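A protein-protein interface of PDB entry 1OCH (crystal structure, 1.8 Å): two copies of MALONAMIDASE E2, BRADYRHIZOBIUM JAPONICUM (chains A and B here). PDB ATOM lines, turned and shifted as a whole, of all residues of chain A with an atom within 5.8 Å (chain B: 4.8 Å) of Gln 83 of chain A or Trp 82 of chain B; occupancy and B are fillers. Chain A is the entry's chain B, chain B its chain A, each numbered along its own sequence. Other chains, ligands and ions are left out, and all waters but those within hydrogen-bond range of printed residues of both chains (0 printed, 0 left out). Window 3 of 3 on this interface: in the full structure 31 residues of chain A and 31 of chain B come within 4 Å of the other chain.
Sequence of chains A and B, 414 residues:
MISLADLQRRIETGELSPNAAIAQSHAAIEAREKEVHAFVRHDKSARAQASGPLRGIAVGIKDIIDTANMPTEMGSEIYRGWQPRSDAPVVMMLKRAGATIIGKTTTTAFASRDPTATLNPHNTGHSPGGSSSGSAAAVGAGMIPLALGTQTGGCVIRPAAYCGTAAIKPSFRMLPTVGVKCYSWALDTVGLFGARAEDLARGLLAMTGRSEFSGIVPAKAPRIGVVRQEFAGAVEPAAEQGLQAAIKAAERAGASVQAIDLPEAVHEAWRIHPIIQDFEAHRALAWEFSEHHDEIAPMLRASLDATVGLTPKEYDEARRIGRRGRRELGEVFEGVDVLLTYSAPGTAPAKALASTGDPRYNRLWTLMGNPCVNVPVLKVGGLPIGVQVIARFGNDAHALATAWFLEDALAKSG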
ATOM      1  N   THR A  67      26.929  -9.145 -26.397  1.00  0.00           N
ATOM      2  CA  THR A  67      26.793  -8.397 -27.638  1.00  0.00           C
ATOM      3  C   THR A  67      25.831  -7.272 -27.279  1.00  0.00           C
ATOM      4  O   THR A  67      24.905  -7.473 -26.491  1.00  0.00           O
ATOM      5  CB  THR A  67      26.216  -9.243 -28.809  1.00  0.00           C
ATOM      6  OG1 THR A  67      25.169 -10.099 -28.336  1.00  0.00           O
ATOM      7  CG2 THR A  67      27.323 -10.079 -29.454  1.00  0.00           C
ATOM      8  N   ALA A  68      26.054  -6.091 -27.845  1.00  0.00           N
ATOM      9  CA  ALA A  68      25.216  -4.940 -27.546  1.00  0.00           C
ATOM     10  C   ALA A  68      23.957  -4.815 -28.406  1.00  0.00           C
ATOM     11  O   ALA A  68      22.977  -4.205 -27.975  1.00  0.00           O
ATOM     12  CB  ALA A  68      26.046  -3.661 -27.665  1.00  0.00           C
ATOM     13  N   ASN A  69      23.989  -5.392 -29.605  1.00  0.00           N
ATOM     14  CA  ASN A  69      22.877  -5.304 -30.555  1.00  0.00           C
ATOM     15  C   ASN A  69      21.995  -6.549 -30.629  1.00  0.00           C
ATOM     16  O   ASN A  69      20.960  -6.540 -31.296  1.00  0.00           O
ATOM     17  CB  ASN A  69      23.430  -4.987 -31.948  1.00  0.00           C
ATOM     18  CG  ASN A  69      24.267  -6.119 -32.510  1.00  0.00           C
ATOM     19  OD1 ASN A  69      25.048  -6.747 -31.788  1.00  0.00           O
ATOM     20  ND2 ASN A  69      24.115  -6.384 -33.803  1.00  0.00           N
ATOM     21  N   MET A  70      22.422  -7.615 -29.960  1.00  0.00           N
ATOM     22  CA  MET A  70      21.684  -8.871 -29.925  1.00  0.00           C
ATOM     23  C   MET A  70      21.667  -9.366 -28.500  1.00  0.00           C
ATOM     24  O   MET A  70      22.594  -9.102 -27.741  1.00  0.00           O
ATOM     25  CB  MET A  70      22.368  -9.940 -30.778  1.00  0.00           C
ATOM     26  CG  MET A  70      22.161  -9.808 -32.246  1.00  0.00           C
ATOM     27  SD  MET A  70      23.182 -11.023 -33.060  1.00  0.00           S
ATOM     28  CE  MET A  70      24.416  -9.966 -33.785  1.00  0.00           C
ATOM     29  N   PRO A  71      20.620 -10.108 -28.122  1.00  0.00           N
ATOM     30  CA  PRO A  71      20.513 -10.639 -26.761  1.00  0.00           C
ATOM     31  C   PRO A  71      21.634 -11.643 -26.442  1.00  0.00           C
ATOM     32  O   PRO A  71      22.248 -12.227 -27.338  1.00  0.00           O
ATOM     33  CB  PRO A  71      19.136 -11.307 -26.759  1.00  0.00           C
ATOM     34  CG  PRO A  71      18.365 -10.525 -27.786  1.00  0.00           C
ATOM     35  CD  PRO A  71      19.383 -10.354 -28.886  1.00  0.00           C
ATOM     36  N   THR A  72      21.900 -11.826 -25.159  1.00  0.00           N
ATOM     37  CA  THR A  72      22.905 -12.781 -24.714  1.00  0.00           C
ATOM     38  C   THR A  72      22.166 -13.534 -23.619  1.00  0.00           C
ATOM     39  O   THR A  72      22.104 -13.077 -22.473  1.00  0.00           O
ATOM     40  CB  THR A  72      24.138 -12.065 -24.147  1.00  0.00           C
ATOM     41  OG1 THR A  72      24.640 -11.141 -25.120  1.00  0.00           O
ATOM     42  CG2 THR A  72      25.228 -13.084 -23.804  1.00  0.00           C
ATOM     43  N   GLY A  81      15.742 -13.088 -23.011  1.00  0.00           N
ATOM     44  CA  GLY A  81      15.619 -11.684 -23.361  1.00  0.00           C
ATOM     45  C   GLY A  81      16.669 -10.750 -22.776  1.00  0.00           C
ATOM     46  O   GLY A  81      16.587  -9.541 -22.977  1.00  0.00           O
ATOM     47  N   TRP A  82      17.653 -11.287 -22.060  1.00  0.00           N
ATOM     48  CA  TRP A  82      18.693 -10.441 -21.473  1.00  0.00           C
ATOM     49  C   TRP A  82      19.498  -9.714 -22.541  1.00  0.00           C
ATOM     50  O   TRP A  82      20.006 -10.329 -23.475  1.00  0.00           O
ATOM     51  CB  TRP A  82      19.653 -11.262 -20.609  1.00  0.00           C
ATOM     52  CG  TRP A  82      20.778 -10.427 -20.066  1.00  0.00           C
ATOM     53  CD1 TRP A  82      22.110 -10.575 -20.322  1.00  0.00           C
ATOM     54  CD2 TRP A  82      20.657  -9.275 -19.219  1.00  0.00           C
ATOM     55  NE1 TRP A  82      22.829  -9.586 -19.690  1.00  0.00           N
ATOM     56  CE2 TRP A  82      21.963  -8.775 -19.006  1.00  0.00           C
ATOM     57  CE3 TRP A  82      19.573  -8.612 -18.624  1.00  0.00           C
ATOM     58  CZ2 TRP A  82      22.215  -7.639 -18.219  1.00  0.00           C
ATOM     59  CZ3 TRP A  82      19.824  -7.481 -17.842  1.00  0.00           C
ATOM     60  CH2 TRP A  82      21.135  -7.008 -17.648  1.00  0.00           C
ATOM     61  N   GLN A  83      19.623  -8.398 -22.391  1.00  0.00           N
ATOM     62  CA  GLN A  83      20.358  -7.600 -23.351  1.00  0.00           C
ATOM     63  C   GLN A  83      21.516  -6.823 -22.730  1.00  0.00           C
ATOM     64  O   GLN A  83      21.306  -5.839 -22.016  1.00  0.00           O
ATOM     65  CB  GLN A  83      19.403  -6.630 -24.056  1.00  0.00           C
ATOM     66  CG  GLN A  83      20.067  -5.750 -25.093  1.00  0.00           C
ATOM     67  CD  GLN A  83      20.883  -6.547 -26.089  1.00  0.00           C
ATOM     68  OE1 GLN A  83      22.116  -6.544 -26.048  1.00  0.00           O
ATOM     69  NE2 GLN A  83      20.200  -7.245 -26.987  1.00  0.00           N
ATOM     70  N   PRO A  84      22.759  -7.277 -22.969  1.00  0.00           N
ATOM     71  CA  PRO A  84      23.937  -6.592 -22.424  1.00  0.00           C
ATOM     72  C   PRO A  84      24.026  -5.178 -22.989  1.00  0.00           C
ATOM     73  O   PRO A  84      23.574  -4.918 -24.104  1.00  0.00           O
ATOM     74  CB  PRO A  84      25.095  -7.468 -22.901  1.00  0.00           C
ATOM     75  CG  PRO A  84      24.498  -8.839 -22.890  1.00  0.00           C
ATOM     76  CD  PRO A  84      23.126  -8.601 -23.506  1.00  0.00           C
ATOM     77  N   ARG A  85      24.606  -4.265 -22.218  1.00  0.00           N
ATOM     78  CA  ARG A  85      24.756  -2.883 -22.658  1.00  0.00           C
ATOM     79  C   ARG A  85      25.888  -2.749 -23.672  1.00  0.00           C
ATOM     80  O   ARG A  85      25.782  -1.996 -24.640  1.00  0.00           O
ATOM     81  CB  ARG A  85      25.040  -1.979 -21.454  1.00  0.00           C
ATOM     82  CG  ARG A  85      25.366  -0.522 -21.790  1.00  0.00           C
ATOM     83  CD  ARG A  85      24.249   0.183 -22.551  1.00  0.00           C
ATOM     84  NE  ARG A  85      24.458   1.631 -22.617  1.00  0.00           N
ATOM     85  CZ  ARG A  85      24.275   2.370 -23.709  1.00  0.00           C
ATOM     86  NH1 ARG A  85      23.881   1.802 -24.841  1.00  0.00           N
ATOM     87  NH2 ARG A  85      24.480   3.684 -23.669  1.00  0.00           N
ATOM     88  N   PRO B  71      20.428   0.137  -9.832  1.00  0.00           N
ATOM     89  CA  PRO B  71      21.225   0.379 -11.039  1.00  0.00           C
ATOM     90  C   PRO B  71      22.732   0.336 -10.741  1.00  0.00           C
ATOM     91  O   PRO B  71      23.156   0.452  -9.592  1.00  0.00           O
ATOM     92  CB  PRO B  71      20.771   1.769 -11.479  1.00  0.00           C
ATOM     93  CG  PRO B  71      19.329   1.810 -11.017  1.00  0.00           C
ATOM     94  CD  PRO B  71      19.426   1.201  -9.635  1.00  0.00           C
ATOM     95  N   THR B  72      23.528   0.149 -11.787  1.00  0.00           N
ATOM     96  CA  THR B  72      24.982   0.120 -11.671  1.00  0.00           C
ATOM     97  C   THR B  72      25.408   1.010 -12.822  1.00  0.00           C
ATOM     98  O   THR B  72      25.547   0.550 -13.955  1.00  0.00           O
ATOM     99  CB  THR B  72      25.525  -1.302 -11.857  1.00  0.00           C
ATOM    100  OG1 THR B  72      24.921  -2.174 -10.891  1.00  0.00           O
ATOM    101  CG2 THR B  72      27.034  -1.317 -11.669  1.00  0.00           C
ATOM    102  N   GLU B  73      25.613   2.291 -12.526  1.00  0.00           N
ATOM    103  CA  GLU B  73      25.921   3.268 -13.560  1.00  0.00           C
ATOM    104  C   GLU B  73      27.380   3.559 -13.916  1.00  0.00           C
ATOM    105  O   GLU B  73      27.661   4.447 -14.724  1.00  0.00           O
ATOM    106  CB  GLU B  73      25.159   4.555 -13.233  1.00  0.00           C
ATOM    107  CG  GLU B  73      23.680   4.264 -12.980  1.00  0.00           C
ATOM    108  CD  GLU B  73      22.860   5.495 -12.648  1.00  0.00           C
ATOM    109  OE1 GLU B  73      23.209   6.199 -11.679  1.00  0.00           O
ATOM    110  OE2 GLU B  73      21.858   5.750 -13.352  1.00  0.00           O
ATOM    111  N   MET B  74      28.297   2.805 -13.322  1.00  0.00           N
ATOM    112  CA  MET B  74      29.720   2.937 -13.623  1.00  0.00           C
ATOM    113  C   MET B  74      30.291   4.348 -13.492  1.00  0.00           C
ATOM    114  O   MET B  74      31.397   4.612 -13.967  1.00  0.00           O
ATOM    115  CB  MET B  74      29.979   2.440 -15.051  1.00  0.00           C
ATOM    116  CG  MET B  74      29.192   1.191 -15.439  1.00  0.00           C
ATOM    117  SD  MET B  74      29.564  -0.232 -14.403  1.00  0.00           S
ATOM    118  CE  MET B  74      28.526  -1.497 -15.184  1.00  0.00           C
ATOM    119  N   TYR B  79      26.194   4.745 -18.920  1.00  0.00           N
ATOM    120  CA  TYR B  79      25.436   3.705 -18.256  1.00  0.00           C
ATOM    121  C   TYR B  79      24.330   4.229 -17.349  1.00  0.00           C
ATOM    122  O   TYR B  79      23.920   3.550 -16.410  1.00  0.00           O
ATOM    123  CB  TYR B  79      26.367   2.799 -17.448  1.00  0.00           C
ATOM    124  CG  TYR B  79      27.231   1.904 -18.303  1.00  0.00           C
ATOM    125  CD1 TYR B  79      28.372   2.395 -18.941  1.00  0.00           C
ATOM    126  CD2 TYR B  79      26.900   0.559 -18.484  1.00  0.00           C
ATOM    127  CE1 TYR B  79      29.167   1.564 -19.736  1.00  0.00           C
ATOM    128  CE2 TYR B  79      27.684  -0.279 -19.278  1.00  0.00           C
ATOM    129  CZ  TYR B  79      28.816   0.228 -19.898  1.00  0.00           C
ATOM    130  OH  TYR B  79      29.604  -0.613 -20.655  1.00  0.00           O
ATOM    131  N   ARG B  80      23.845   5.433 -17.629  1.00  0.00           N
ATOM    132  CA  ARG B  80      22.770   6.008 -16.825  1.00  0.00           C
ATOM    133  C   ARG B  80      21.558   5.082 -16.859  1.00  0.00           C
ATOM    134  O   ARG B  80      21.103   4.681 -17.928  1.00  0.00           O
ATOM    135  CB  ARG B  80      22.377   7.380 -17.367  1.00  0.00           C
ATOM    136  CG  ARG B  80      21.217   8.028 -16.628  1.00  0.00           C
ATOM    137  CD  ARG B  80      20.742   9.271 -17.357  1.00  0.00           C
ATOM    138  NE  ARG B  80      19.686   9.969 -16.631  1.00  0.00           N
ATOM    139  CZ  ARG B  80      19.074  11.064 -17.073  1.00  0.00           C
ATOM    140  NH1 ARG B  80      19.412  11.590 -18.246  1.00  0.00           N
ATOM    141  NH2 ARG B  80      18.127  11.636 -16.338  1.00  0.00           N
ATOM    142  N   GLY B  81      21.050   4.734 -15.682  1.00  0.00           N
ATOM    143  CA  GLY B  81      19.894   3.859 -15.600  1.00  0.00           C
ATOM    144  C   GLY B  81      20.145   2.382 -15.874  1.00  0.00           C
ATOM    145  O   GLY B  81      19.219   1.580 -15.789  1.00  0.00           O
ATOM    146  N   TRP B  82      21.382   2.013 -16.200  1.00  0.00           N
ATOM    147  CA  TRP B  82      21.716   0.610 -16.484  1.00  0.00           C
ATOM    148  C   TRP B  82      21.393  -0.306 -15.310  1.00  0.00           C
ATOM    149  O   TRP B  82      21.808  -0.052 -14.179  1.00  0.00           O
ATOM    150  CB  TRP B  82      23.200   0.472 -16.848  1.00  0.00           C
ATOM    151  CG  TRP B  82      23.653  -0.960 -17.006  1.00  0.00           C
ATOM    152  CD1 TRP B  82      24.586  -1.610 -16.249  1.00  0.00           C
ATOM    153  CD2 TRP B  82      23.167  -1.922 -17.954  1.00  0.00           C
ATOM    154  NE1 TRP B  82      24.711  -2.913 -16.664  1.00  0.00           N
ATOM    155  CE2 TRP B  82      23.853  -3.134 -17.707  1.00  0.00           C
ATOM    156  CE3 TRP B  82      22.217  -1.880 -18.986  1.00  0.00           C
ATOM    157  CZ2 TRP B  82      23.620  -4.298 -18.456  1.00  0.00           C
ATOM    158  CZ3 TRP B  82      21.986  -3.042 -19.733  1.00  0.00           C
ATOM    159  CH2 TRP B  82      22.686  -4.230 -19.461  1.00  0.00           C
ATOM    160  N   GLN B  83      20.669  -1.386 -15.588  1.00  0.00           N
ATOM    161  CA  GLN B  83      20.282  -2.316 -14.544  1.00  0.00           C
ATOM    162  C   GLN B  83      20.742  -3.747 -14.794  1.00  0.00           C
ATOM    163  O   GLN B  83      20.181  -4.451 -15.639  1.00  0.00           O
ATOM    164  CB  GLN B  83      18.756  -2.293 -14.372  1.00  0.00           C
ATOM    165  CG  GLN B  83      18.227  -3.179 -13.252  1.00  0.00           C
ATOM    166  CD  GLN B  83      18.937  -2.927 -11.936  1.00  0.00           C
ATOM    167  OE1 GLN B  83      19.775  -3.718 -11.505  1.00  0.00           O
ATOM    168  NE2 GLN B  83      18.619  -1.810 -11.301  1.00  0.00           N
ATOM    169  N   PRO B  84      21.771  -4.199 -14.060  1.00  0.00           N
ATOM    170  CA  PRO B  84      22.272  -5.567 -14.231  1.00  0.00           C
ATOM    171  C   PRO B  84      21.196  -6.577 -13.829  1.00  0.00           C
ATOM    172  O   PRO B  84      20.382  -6.311 -12.943  1.00  0.00           O
ATOM    173  CB  PRO B  84      23.472  -5.618 -13.291  1.00  0.00           C
ATOM    174  CG  PRO B  84      23.939  -4.189 -13.257  1.00  0.00           C
ATOM    175  CD  PRO B  84      22.643  -3.436 -13.149  1.00  0.00           C
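N of Thr 72 of chain B is in hydrogen-bond range of O of Trp 82 of chain B, 3.0 Å away. The backbone carbonyl oxygen (O) of Thr 67 of chain A lies close to the side-chain amide oxygen (OE1) of Gln 83 of chain A. The side-chain amide oxygen (OE1) of Gln 83 of chain A lies close to the backbone carbonyl oxygen (O) of Ala 68 of chain A (3.2 Å). The backbone carbonyl oxygen of Met 70 of chain A sits close to the side-chain amide oxygen of Gln 83 of chain A, at 3.1 Å. The backbone NH of Thr 72 of chain A lies within hydrogen-bond range of the backbone carbonyl oxygen of Trp 82 of chain A (2.9 Å).
Among the printed residues, pairs that only touch across the chains: Trp 82 of chain A with Trp 82 of chain B, Trp 82 of chain A with Gln 83 of chain B, Trp 82 of chain A with Pro 84 of chain B, Gln 83 of chain A with Trp 82 of chain B, Pro 84 of chain A with Trp 82 of chain B, Arg 85 of chain A with Tyr 79 of chain B and Arg 85 of chain A with Trp 82 of chain B.
Trp 82 of chain B touches just these residues of chain A: Trp 82 (3.6 Å), Gln 83 (3.3 Å), Pro 84 (3.9 Å) and Arg 85 (3.4 Å). Of the printed residues of chain A, Tyr 79 of chain B touches Arg 85. Printed residues of chain A within 4 Å of Pro 84 of chain B: Trp 82 (3.8 Å). Of the printed residues of chain B, Pro 84 of chain A touches Trp 82 (3.9 Å). Gly 81 of chain B touches none of the printed residues of chain A. Met 70 of chain A touches none of the printed residues of chain B. The nearest printed residue of chain A that does not touch Trp 82 of chain B is Thr 67 of chain A (8.1 Å). The nearest printed residue of chain B that does not touch Trp 82 of chain A is Gly 81 of chain B (9.0 Å).
Hydrophobic or aromatic side chains of chain A within 4 Å of the printed part of chain B: Trp 82.
Trp 82 of chain A touches its own counterpart, Trp 82 of chain B. Trp 82 of chain A touches Gln 83 of chain B, and with the chains exchanged Gln 83 of chain A touches Trp 82 of chain B. Trp 82 of chain A touches Pro 84 of chain B, and with the chains exchanged Pro 84 of chain A touches Trp 82 of chain B. Positions printed for both chains: 71, 72, 81, 82, 83 and 84. Of the 7 pairs that touch across the chains among the printed residues, 5 have their exchanged pair printed and touching as well.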
